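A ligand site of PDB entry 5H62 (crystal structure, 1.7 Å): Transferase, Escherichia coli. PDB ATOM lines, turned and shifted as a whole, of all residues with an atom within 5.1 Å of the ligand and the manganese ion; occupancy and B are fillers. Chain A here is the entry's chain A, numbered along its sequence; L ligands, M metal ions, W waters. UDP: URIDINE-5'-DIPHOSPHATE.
The backbone carbonyl oxygen (O) of Phe 66 lies within hydrogen-bond range of a nitrogen (N3) of the ligand, 2.8 Å away.
An oxygen (O2A) of the ligand lies within hydrogen-bond range of the side-chain hydroxyl (OG) of Ser 346 (2.7 Å).
The backbone carbonyl oxygen (O) of Gln 64 is in hydrogen-bond range of an oxygen (O2') of the ligand (2.7 Å).
NE1 of Trp 347 is in hydrogen-bond range of O3A of the ligand (3.3 Å).
The backbone NH (N) of Ala 240 is in hydrogen-bond range of an oxygen (O3') of the ligand (3.0 Å).
The backbone NH (N) of Phe 66 sits at hydrogen-bond distance from an oxygen (O2) of the ligand (2.9 Å).
An oxygen (O2A) of the ligand sits at hydrogen-bond distance from the side-chain hydroxyl (OH) of Tyr 88 (2.8 Å).
The side-chain hydroxyl (OG) of Ser 345 is in hydrogen-bond range of an oxygen (O1B) of the ligand, 2.8 Å away.
OH of Tyr 237 is in hydrogen-bond range of O2' of the ligand, 3.3 Å away.
The guanidinium group of Arg 207 is in hydrogen-bond range of an oxygen (O4') of the ligand, at 3.4 Å.
NE of Arg 348 lies within salt-bridge range of O1B of the ligand (2.9 Å).
O2A of the ligand lies within hydrogen-bond range of N of Ser 346 (3.0 Å).
The side-chain carboxylate (OD1) of Asp 239 lies within salt-bridge range of the guanidinium group (NH1) of Arg 207 (3.2 Å).
The guanidinium group (NH2) of Arg 207 lies close to the side-chain hydroxyl (OH) of Tyr 237 (3.1 Å).
The guanidinium group (NE) of Arg 207 is in hydrogen-bond range of the side-chain amide oxygen (OE1) of Gln 64.
The side-chain hydroxyl (OG1) of Thr 339 lies within hydrogen-bond range of the backbone carbonyl oxygen (O) of Asp 241 (2.8 Å).
OH of Tyr 88 is in hydrogen-bond range of ND2 of Asn 86, at 3.0 Å.
OH of Tyr 237 lies within hydrogen-bond range of OD1 of Asp 239, at 2.7 Å.
The indole nitrogen of Trp 65 lies within hydrogen-bond range of the side-chain carboxylate of Glu 67.
The side-chain hydroxyl (OG) of Ser 345 is in hydrogen-bond range of the backbone NH (N) of Trp 347 (3.1 Å).
Merely in contact with the ligand: Trp 65, Phe 203 and Asp 239.
16 residues have an atom within 4 Å of the ligand: Gln 64, Trp 65, Phe 66, Tyr 88, Phe 203, Arg 207, Tyr 237, Asp 239, Ala 240, Asp 241, Asn 338, Ser 340, Ser 345, Ser 346, Trp 347 and Arg 348.
Along chain A the residues within 4 Å of the ligand span positions 64 to 348.
The nearest printed residue that does not touch the ligand is Asn 86 (4.5 Å).
Within 4 Å of the manganese ion: Asp 241, Asn 338 and Ser 340.
The manganese ion is bound by water W4 (2.1 Å), an oxygen (O2B) of the ligand (2.1 Å), an oxygen (O1A) of the ligand (2.2 Å), the side-chain amide oxygen (OD1) of Asn 338 (2.2 Å), the side-chain carboxylate (OD2) of Asp 241 (2.2 Å) and the side-chain hydroxyl (OG) of Ser 340 (2.3 Å).
Water W4 lies within hydrogen-bond range of the side-chain carboxylate (OD1) of Asp 241 (2.7 Å) and the side-chain carboxylate (OD2) of Asp 239 (2.7 Å).
Water W3 bridges O3B of the ligand and NE1 of Trp 347.
Water W5 lies within hydrogen-bond range of an oxygen (O3') of the ligand (2.9 Å), the backbone NH of Asp 241 (3.0 Å), the backbone NH of Ala 240 (3.3 Å) and the side-chain hydroxyl of Tyr 88 (3.4 Å).
Water W1 lies within hydrogen-bond range of an oxygen (O4) of the ligand (2.8 Å) and the backbone carbonyl oxygen (O) of Phe 66 (3.4 Å).
Water W2 bridges the backbone carbonyl oxygen (O) of Ser 346 and an oxygen (O4) of the ligand.
Water W7 lies within hydrogen-bond range of the backbone NH of Gln 64 (2.8 Å), the side-chain hydroxyl of Tyr 237 (2.9 Å), an oxygen (O2') of the ligand (3.1 Å) and the backbone NH of Ala 240 (3.3 Å).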
ATOM      1  N   GLN A  64      -1.979  24.071 -26.446  1.00  0.00           N
ATOM      2  CA  GLN A  64      -2.800  25.080 -25.815  1.00  0.00           C
ATOM      3  C   GLN A  64      -2.061  25.764 -24.680  1.00  0.00           C
ATOM      4  O   GLN A  64      -1.392  25.037 -23.912  1.00  0.00           O
ATOM      5  CB  GLN A  64      -4.055  24.404 -25.280  1.00  0.00           C
ATOM      6  CG  GLN A  64      -4.991  25.313 -24.499  1.00  0.00           C
ATOM      7  CD  GLN A  64      -6.177  24.554 -23.957  1.00  0.00           C
ATOM      8  OE1 GLN A  64      -6.098  23.411 -23.566  1.00  0.00           O
ATOM      9  NE2 GLN A  64      -7.372  25.250 -23.930  1.00  0.00           N
ATOM     10  N   TRP A  65      -2.066  27.082 -24.612  1.00  0.00           N
ATOM     11  CA  TRP A  65      -1.586  27.728 -23.390  1.00  0.00           C
ATOM     12  C   TRP A  65      -2.552  28.872 -23.002  1.00  0.00           C
ATOM     13  O   TRP A  65      -2.556  29.914 -23.621  1.00  0.00           O
ATOM     14  CB  TRP A  65      -0.115  28.210 -23.475  1.00  0.00           C
ATOM     15  CG  TRP A  65       0.343  28.562 -22.119  1.00  0.00           C
ATOM     16  CD1 TRP A  65       0.479  29.842 -21.590  1.00  0.00           C
ATOM     17  CD2 TRP A  65       0.571  27.669 -21.047  1.00  0.00           C
ATOM     18  NE1 TRP A  65       0.827  29.737 -20.261  1.00  0.00           N
ATOM     19  CE2 TRP A  65       0.866  28.420 -19.932  1.00  0.00           C
ATOM     20  CE3 TRP A  65       0.514  26.270 -20.905  1.00  0.00           C
ATOM     21  CZ2 TRP A  65       1.127  27.878 -18.699  1.00  0.00           C
ATOM     22  CZ3 TRP A  65       0.776  25.729 -19.671  1.00  0.00           C
ATOM     23  CH2 TRP A  65       1.114  26.556 -18.588  1.00  0.00           C
ATOM     24  N   PHE A  66      -3.310  28.612 -21.942  1.00  0.00           N
ATOM     25  CA  PHE A  66      -4.235  29.580 -21.391  1.00  0.00           C
ATOM     26  C   PHE A  66      -3.562  30.103 -20.162  1.00  0.00           C
ATOM     27  O   PHE A  66      -3.329  29.352 -19.202  1.00  0.00           O
ATOM     28  CB  PHE A  66      -5.598  28.923 -21.090  1.00  0.00           C
ATOM     29  CG  PHE A  66      -6.529  28.818 -22.251  1.00  0.00           C
ATOM     30  CD1 PHE A  66      -6.078  28.743 -23.529  1.00  0.00           C
ATOM     31  CD2 PHE A  66      -7.865  28.874 -22.035  1.00  0.00           C
ATOM     32  CE1 PHE A  66      -6.938  28.709 -24.621  1.00  0.00           C
ATOM     33  CE2 PHE A  66      -8.777  28.802 -23.081  1.00  0.00           C
ATOM     34  CZ  PHE A  66      -8.352  28.723 -24.406  1.00  0.00           C
ATOM     35  N   GLU A  67      -3.285  31.390 -20.129  1.00  0.00           N
ATOM     36  CA  GLU A  67      -2.463  31.964 -19.077  1.00  0.00           C
ATOM     37  C   GLU A  67      -3.274  32.909 -18.209  1.00  0.00           C
ATOM     38  O   GLU A  67      -3.693  33.968 -18.667  1.00  0.00           O
ATOM     39  CB  GLU A  67      -1.289  32.706 -19.707  1.00  0.00           C
ATOM     40  CG  GLU A  67      -0.417  33.412 -18.708  1.00  0.00           C
ATOM     41  CD  GLU A  67       0.097  32.471 -17.690  1.00  0.00           C
ATOM     42  OE1 GLU A  67      -0.129  32.764 -16.469  1.00  0.00           O
ATOM     43  OE2 GLU A  67       0.746  31.446 -18.035  1.00  0.00           O
ATOM     44  N   ARG A  72       3.095  37.722 -14.984  1.00  0.00           N
ATOM     45  CA  ARG A  72       4.284  37.065 -14.462  1.00  0.00           C
ATOM     46  C   ARG A  72       5.416  36.907 -15.483  1.00  0.00           C
ATOM     47  O   ARG A  72       6.521  36.523 -15.136  1.00  0.00           O
ATOM     48  CB  ARG A  72       3.942  35.707 -13.852  1.00  0.00           C
ATOM     49  CG  ARG A  72       3.566  34.582 -14.840  1.00  0.00           C
ATOM     50  CD  ARG A  72       2.937  33.384 -14.117  1.00  0.00           C
ATOM     51  NE  ARG A  72       2.462  32.359 -15.038  1.00  0.00           N
ATOM     52  CZ  ARG A  72       2.693  31.043 -14.944  1.00  0.00           C
ATOM     53  NH1 ARG A  72       3.403  30.539 -13.918  1.00  0.00           N
ATOM     54  NH2 ARG A  72       2.165  30.208 -15.864  1.00  0.00           N
ATOM     55  N   ASN A  86       8.815  22.839 -16.271  1.00  0.00           N
ATOM     56  CA  ASN A  86       7.779  22.897 -17.294  1.00  0.00           C
ATOM     57  C   ASN A  86       8.235  23.688 -18.497  1.00  0.00           C
ATOM     58  O   ASN A  86       7.795  24.830 -18.773  1.00  0.00           O
ATOM     59  CB  ASN A  86       6.510  23.518 -16.706  1.00  0.00           C
ATOM     60  CG  ASN A  86       5.995  22.742 -15.517  1.00  0.00           C
ATOM     61  OD1 ASN A  86       6.180  23.187 -14.386  1.00  0.00           O
ATOM     62  ND2 ASN A  86       5.399  21.593 -15.736  1.00  0.00           N
ATOM     63  N   TYR A  88       7.579  24.197 -21.459  1.00  0.00           N
ATOM     64  CA  TYR A  88       6.589  23.969 -22.453  1.00  0.00           C
ATOM     65  C   TYR A  88       6.730  24.696 -23.782  1.00  0.00           C
ATOM     66  O   TYR A  88       6.466  24.128 -24.856  1.00  0.00           O
ATOM     67  CB  TYR A  88       5.200  24.220 -21.855  1.00  0.00           C
ATOM     68  CG  TYR A  88       4.788  23.210 -20.790  1.00  0.00           C
ATOM     69  CD1 TYR A  88       5.574  22.081 -20.464  1.00  0.00           C
ATOM     70  CD2 TYR A  88       3.591  23.354 -20.127  1.00  0.00           C
ATOM     71  CE1 TYR A  88       5.186  21.203 -19.490  1.00  0.00           C
ATOM     72  CE2 TYR A  88       3.197  22.429 -19.174  1.00  0.00           C
ATOM     73  CZ  TYR A  88       4.010  21.386 -18.859  1.00  0.00           C
ATOM     74  OH  TYR A  88       3.655  20.510 -17.881  1.00  0.00           O
ATOM     75  N   PHE A 203      -9.219  25.957 -19.410  1.00  0.00           N
ATOM     76  CA  PHE A 203      -8.593  25.322 -20.561  1.00  0.00           C
ATOM     77  C   PHE A 203      -9.241  24.052 -20.944  1.00  0.00           C
ATOM     78  O   PHE A 203      -9.327  23.764 -22.141  1.00  0.00           O
ATOM     79  CB  PHE A 203      -7.035  25.188 -20.465  1.00  0.00           C
ATOM     80  CG  PHE A 203      -6.497  24.789 -19.135  1.00  0.00           C
ATOM     81  CD1 PHE A 203      -6.058  25.749 -18.258  1.00  0.00           C
ATOM     82  CD2 PHE A 203      -6.273  23.464 -18.822  1.00  0.00           C
ATOM     83  CE1 PHE A 203      -5.417  25.402 -17.026  1.00  0.00           C
ATOM     84  CE2 PHE A 203      -5.644  23.127 -17.652  1.00  0.00           C
ATOM     85  CZ  PHE A 203      -5.257  24.106 -16.719  1.00  0.00           C
ATOM     86  N   ARG A 207     -10.663  23.629 -24.771  1.00  0.00           N
ATOM     87  CA  ARG A 207      -9.995  22.584 -25.568  1.00  0.00           C
ATOM     88  C   ARG A 207     -11.004  21.786 -26.322  1.00  0.00           C
ATOM     89  O   ARG A 207     -10.830  21.545 -27.484  1.00  0.00           O
ATOM     90  CB  ARG A 207      -9.215  21.664 -24.614  1.00  0.00           C
ATOM     91  CG  ARG A 207      -8.370  20.641 -25.276  1.00  0.00           C
ATOM     92  CD  ARG A 207      -7.624  19.825 -24.244  1.00  0.00           C
ATOM     93  NE  ARG A 207      -6.729  20.660 -23.481  1.00  0.00           N
ATOM     94  CZ  ARG A 207      -6.023  20.261 -22.424  1.00  0.00           C
ATOM     95  NH1 ARG A 207      -6.035  19.025 -22.001  1.00  0.00           N
ATOM     96  NH2 ARG A 207      -5.316  21.149 -21.726  1.00  0.00           N
ATOM     97  N   TYR A 237      -4.552  17.320 -30.976  1.00  0.00           N
ATOM     98  CA  TYR A 237      -4.316  18.135 -29.803  1.00  0.00           C
ATOM     99  C   TYR A 237      -3.378  17.384 -28.884  1.00  0.00           C
ATOM    100  O   TYR A 237      -3.642  16.173 -28.543  1.00  0.00           O
ATOM    101  CB  TYR A 237      -5.624  18.490 -29.032  1.00  0.00           C
ATOM    102  CG  TYR A 237      -5.258  19.054 -27.715  1.00  0.00           C
ATOM    103  CD1 TYR A 237      -4.805  20.352 -27.638  1.00  0.00           C
ATOM    104  CD2 TYR A 237      -5.081  18.220 -26.596  1.00  0.00           C
ATOM    105  CE1 TYR A 237      -4.275  20.872 -26.470  1.00  0.00           C
ATOM    106  CE2 TYR A 237      -4.564  18.706 -25.450  1.00  0.00           C
ATOM    107  CZ  TYR A 237      -4.122  20.038 -25.379  1.00  0.00           C
ATOM    108  OH  TYR A 237      -3.558  20.535 -24.221  1.00  0.00           O
ATOM    109  N   ASP A 239      -1.124  17.959 -25.055  1.00  0.00           N
ATOM    110  CA  ASP A 239      -0.521  18.688 -23.950  1.00  0.00           C
ATOM    111  C   ASP A 239       0.959  18.970 -24.275  1.00  0.00           C
ATOM    112  O   ASP A 239       1.591  18.142 -24.976  1.00  0.00           O
ATOM    113  CB  ASP A 239      -0.586  17.881 -22.677  1.00  0.00           C
ATOM    114  CG  ASP A 239      -1.938  17.962 -21.980  1.00  0.00           C
ATOM    115  OD1 ASP A 239      -2.852  18.674 -22.461  1.00  0.00           O
ATOM    116  OD2 ASP A 239      -2.069  17.317 -20.874  1.00  0.00           O
ATOM    117  N   ALA A 240       1.475  20.106 -23.815  1.00  0.00           N
ATOM    118  CA  ALA A 240       2.844  20.525 -24.111  1.00  0.00           C
ATOM    119  C   ALA A 240       3.919  19.662 -23.520  1.00  0.00           C
ATOM    120  O   ALA A 240       5.048  19.689 -24.011  1.00  0.00           O
ATOM    121  CB  ALA A 240       3.031  21.978 -23.778  1.00  0.00           C
ATOM    122  N   ASP A 241       3.579  18.812 -22.590  1.00  0.00           N
ATOM    123  CA  ASP A 241       4.483  17.796 -22.046  1.00  0.00           C
ATOM    124  C   ASP A 241       4.470  16.448 -22.744  1.00  0.00           C
ATOM    125  O   ASP A 241       5.085  15.503 -22.276  1.00  0.00           O
ATOM    126  CB  ASP A 241       4.239  17.613 -20.552  1.00  0.00           C
ATOM    127  CG  ASP A 241       3.000  16.883 -20.266  1.00  0.00           C
ATOM    128  OD1 ASP A 241       2.197  16.622 -21.157  1.00  0.00           O
ATOM    129  OD2 ASP A 241       2.835  16.541 -19.102  1.00  0.00           O
ATOM    130  N   ASN A 338       2.826  12.668 -21.111  1.00  0.00           N
ATOM    131  CA  ASN A 338       2.614  13.244 -19.814  1.00  0.00           C
ATOM    132  C   ASN A 338       3.847  13.377 -18.950  1.00  0.00           C
ATOM    133  O   ASN A 338       3.869  12.964 -17.800  1.00  0.00           O
ATOM    134  CB  ASN A 338       1.533  12.468 -19.078  1.00  0.00           C
ATOM    135  CG  ASN A 338       0.960  13.192 -17.891  1.00  0.00           C
ATOM    136  OD1 ASN A 338       1.253  14.340 -17.617  1.00  0.00           O
ATOM    137  ND2 ASN A 338       0.239  12.475 -17.117  1.00  0.00           N
ATOM    138  N   THR A 339       4.875  14.015 -19.527  1.00  0.00           N
ATOM    139  CA  THR A 339       6.099  14.147 -18.765  1.00  0.00           C
ATOM    140  C   THR A 339       6.047  15.006 -17.559  1.00  0.00           C
ATOM    141  O   THR A 339       6.912  14.892 -16.715  1.00  0.00           O
ATOM    142  CB  THR A 339       7.327  14.508 -19.656  1.00  0.00           C
ATOM    143  OG1 THR A 339       7.099  15.775 -20.298  1.00  0.00           O
ATOM    144  CG2 THR A 339       7.545  13.532 -20.689  1.00  0.00           C
ATOM    145  N   SER A 340       4.998  15.849 -17.366  1.00  0.00           N
ATOM    146  CA  SER A 340       4.876  16.601 -16.200  1.00  0.00           C
ATOM    147  C   SER A 340       4.709  15.665 -15.010  1.00  0.00           C
ATOM    148  O   SER A 340       5.028  16.046 -13.928  1.00  0.00           O
ATOM    149  CB  SER A 340       3.666  17.557 -16.233  1.00  0.00           C
ATOM    150  OG  SER A 340       2.466  16.812 -16.176  1.00  0.00           O
ATOM    151  N   SER A 341       4.154  14.480 -15.238  1.00  0.00           N
ATOM    152  CA  SER A 341       3.943  13.565 -14.149  1.00  0.00           C
ATOM    153  C   SER A 341       5.241  13.090 -13.535  1.00  0.00           C
ATOM    154  O   SER A 341       5.282  12.617 -12.427  1.00  0.00           O
ATOM    155  CB  SER A 341       3.084  12.398 -14.553  1.00  0.00           C
ATOM    156  OG  SER A 341       3.615  11.642 -15.614  1.00  0.00           O
ATOM    157  N   ALA A 344       6.740  18.134 -12.463  1.00  0.00           N
ATOM    158  CA  ALA A 344       5.583  18.633 -11.702  1.00  0.00           C
ATOM    159  C   ALA A 344       4.508  19.190 -12.623  1.00  0.00           C
ATOM    160  O   ALA A 344       4.793  19.707 -13.664  1.00  0.00           O
ATOM    161  CB  ALA A 344       6.001  19.693 -10.707  1.00  0.00           C
ATOM    162  N   SER A 345       3.275  19.119 -12.180  1.00  0.00           N
ATOM    163  CA  SER A 345       2.167  19.700 -12.957  1.00  0.00           C
ATOM    164  C   SER A 345       2.345  21.190 -13.012  1.00  0.00           C
ATOM    165  O   SER A 345       2.836  21.841 -12.060  1.00  0.00           O
ATOM    166  CB  SER A 345       0.879  19.423 -12.239  1.00  0.00           C
ATOM    167  OG  SER A 345      -0.182  20.165 -12.828  1.00  0.00           O
ATOM    168  N   SER A 346       1.975  21.786 -14.117  1.00  0.00           N
ATOM    169  CA  SER A 346       2.100  23.252 -14.201  1.00  0.00           C
ATOM    170  C   SER A 346       0.978  24.009 -13.528  1.00  0.00           C
ATOM    171  O   SER A 346       0.948  25.262 -13.628  1.00  0.00           O
ATOM    172  CB  SER A 346       2.142  23.647 -15.656  1.00  0.00           C
ATOM    173  OG  SER A 346       0.907  23.220 -16.275  1.00  0.00           O
ATOM    174  N   TRP A 347       0.016  23.283 -12.963  1.00  0.00           N
ATOM    175  CA  TRP A 347      -1.132  23.929 -12.294  1.00  0.00           C
ATOM    176  C   TRP A 347      -1.664  23.222 -11.066  1.00  0.00           C
ATOM    177  O   TRP A 347      -2.278  23.881 -10.241  1.00  0.00           O
ATOM    178  CB  TRP A 347      -2.293  24.148 -13.300  1.00  0.00           C
ATOM    179  CG  TRP A 347      -2.932  22.902 -13.793  1.00  0.00           C
ATOM    180  CD1 TRP A 347      -2.539  22.155 -14.907  1.00  0.00           C
ATOM    181  CD2 TRP A 347      -4.019  22.176 -13.210  1.00  0.00           C
ATOM    182  NE1 TRP A 347      -3.333  21.087 -15.041  1.00  0.00           N
ATOM    183  CE2 TRP A 347      -4.239  21.060 -14.006  1.00  0.00           C
ATOM    184  CE3 TRP A 347      -4.851  22.384 -12.089  1.00  0.00           C
ATOM    185  CZ2 TRP A 347      -5.252  20.126 -13.743  1.00  0.00           C
ATOM    186  CZ3 TRP A 347      -5.845  21.476 -11.823  1.00  0.00           C
ATOM    187  CH2 TRP A 347      -6.041  20.345 -12.651  1.00  0.00           C
ATOM    188  N   ARG A 348      -1.500  21.911 -10.901  1.00  0.00           N
ATOM    189  CA  ARG A 348      -2.138  21.220  -9.742  1.00  0.00           C
ATOM    190  C   ARG A 348      -1.646  21.634  -8.352  1.00  0.00           C
ATOM    191  O   ARG A 348      -0.482  21.970  -8.240  1.00  0.00           O
ATOM    192  CB  ARG A 348      -1.967  19.738  -9.833  1.00  0.00           C
ATOM    193  CG  ARG A 348      -2.859  19.149 -10.903  1.00  0.00           C
ATOM    194  CD  ARG A 348      -2.509  17.702 -11.150  1.00  0.00           C
ATOM    195  NE  ARG A 348      -3.073  17.335 -12.437  1.00  0.00           N
ATOM    196  CZ  ARG A 348      -4.329  16.971 -12.653  1.00  0.00           C
ATOM    197  NH1 ARG A 348      -5.210  16.929 -11.650  1.00  0.00           N
ATOM    198  NH2 ARG A 348      -4.742  16.691 -13.876  1.00  0.00           N
HETATM  199  N1  UDP L   1      -2.541  24.440 -19.184  1.00  0.00           N
HETATM  200  C2  UDP L   1      -2.835  25.783 -19.511  1.00  0.00           C
HETATM  201  N3  UDP L   1      -2.577  26.747 -18.670  1.00  0.00           N
HETATM  202  C4  UDP L   1      -2.061  26.475 -17.466  1.00  0.00           C
HETATM  203  C5  UDP L   1      -1.693  25.191 -17.110  1.00  0.00           C
HETATM  204  C6  UDP L   1      -1.938  24.175 -17.973  1.00  0.00           C
HETATM  205  O2  UDP L   1      -3.333  26.026 -20.640  1.00  0.00           O
HETATM  206  O4  UDP L   1      -1.770  27.463 -16.706  1.00  0.00           O
HETATM  207  C1' UDP L   1      -2.887  23.416 -20.207  1.00  0.00           C
HETATM  208  C2' UDP L   1      -1.747  23.281 -21.213  1.00  0.00           C
HETATM  209  O2' UDP L   1      -2.392  23.037 -22.450  1.00  0.00           O
HETATM  210  C3' UDP L   1      -0.910  22.157 -20.669  1.00  0.00           C
HETATM  211  C4' UDP L   1      -2.036  21.227 -20.133  1.00  0.00           C
HETATM  212  O4' UDP L   1      -2.935  22.162 -19.507  1.00  0.00           O
HETATM  213  O3' UDP L   1      -0.239  21.480 -21.756  1.00  0.00           O
HETATM  214  C5' UDP L   1      -1.604  20.168 -19.130  1.00  0.00           C
HETATM  215  O5' UDP L   1      -0.677  20.773 -18.213  1.00  0.00           O
HETATM  216  PA  UDP L   1       0.204  19.735 -17.352  1.00  0.00           P
HETATM  217  O1A UDP L   1       0.711  18.645 -18.271  1.00  0.00           O
HETATM  218  O2A UDP L   1       1.161  20.595 -16.717  1.00  0.00           O
HETATM  219  O3A UDP L   1      -0.888  19.199 -16.302  1.00  0.00           O
HETATM  220  PB  UDP L   1      -1.291  17.765 -15.731  1.00  0.00           P
HETATM  221  O1B UDP L   1      -0.912  17.889 -14.307  1.00  0.00           O
HETATM  222  O2B UDP L   1      -0.584  16.697 -16.487  1.00  0.00           O
HETATM  223  O3B UDP L   1      -2.769  17.665 -15.978  1.00  0.00           O
HETATM  224 MN    MN M   1       0.970  16.508 -17.894  1.00  0.00          MN
HETATM  225  O   HOH W   1      -2.859  29.870 -15.923  1.00  0.00           O
HETATM  226  O   HOH W   2       0.288  27.436 -14.799  1.00  0.00           O
HETATM  227  O   HOH W   3      -4.558  19.166 -17.280  1.00  0.00           O
HETATM  228  O   HOH W   4       0.018  16.055 -19.714  1.00  0.00           O
HETATM  229  O   HOH W   5       1.699  19.777 -20.527  1.00  0.00           O
HETATM  230  O   HOH W   6       1.442  16.667 -13.926  1.00  0.00           O
HETATM  231  O   HOH W   7      -1.074  21.825 -24.957  1.00  0.00           O
HETATM  232  O   HOH W   8      -0.634  14.305 -14.994  1.00  0.00           O
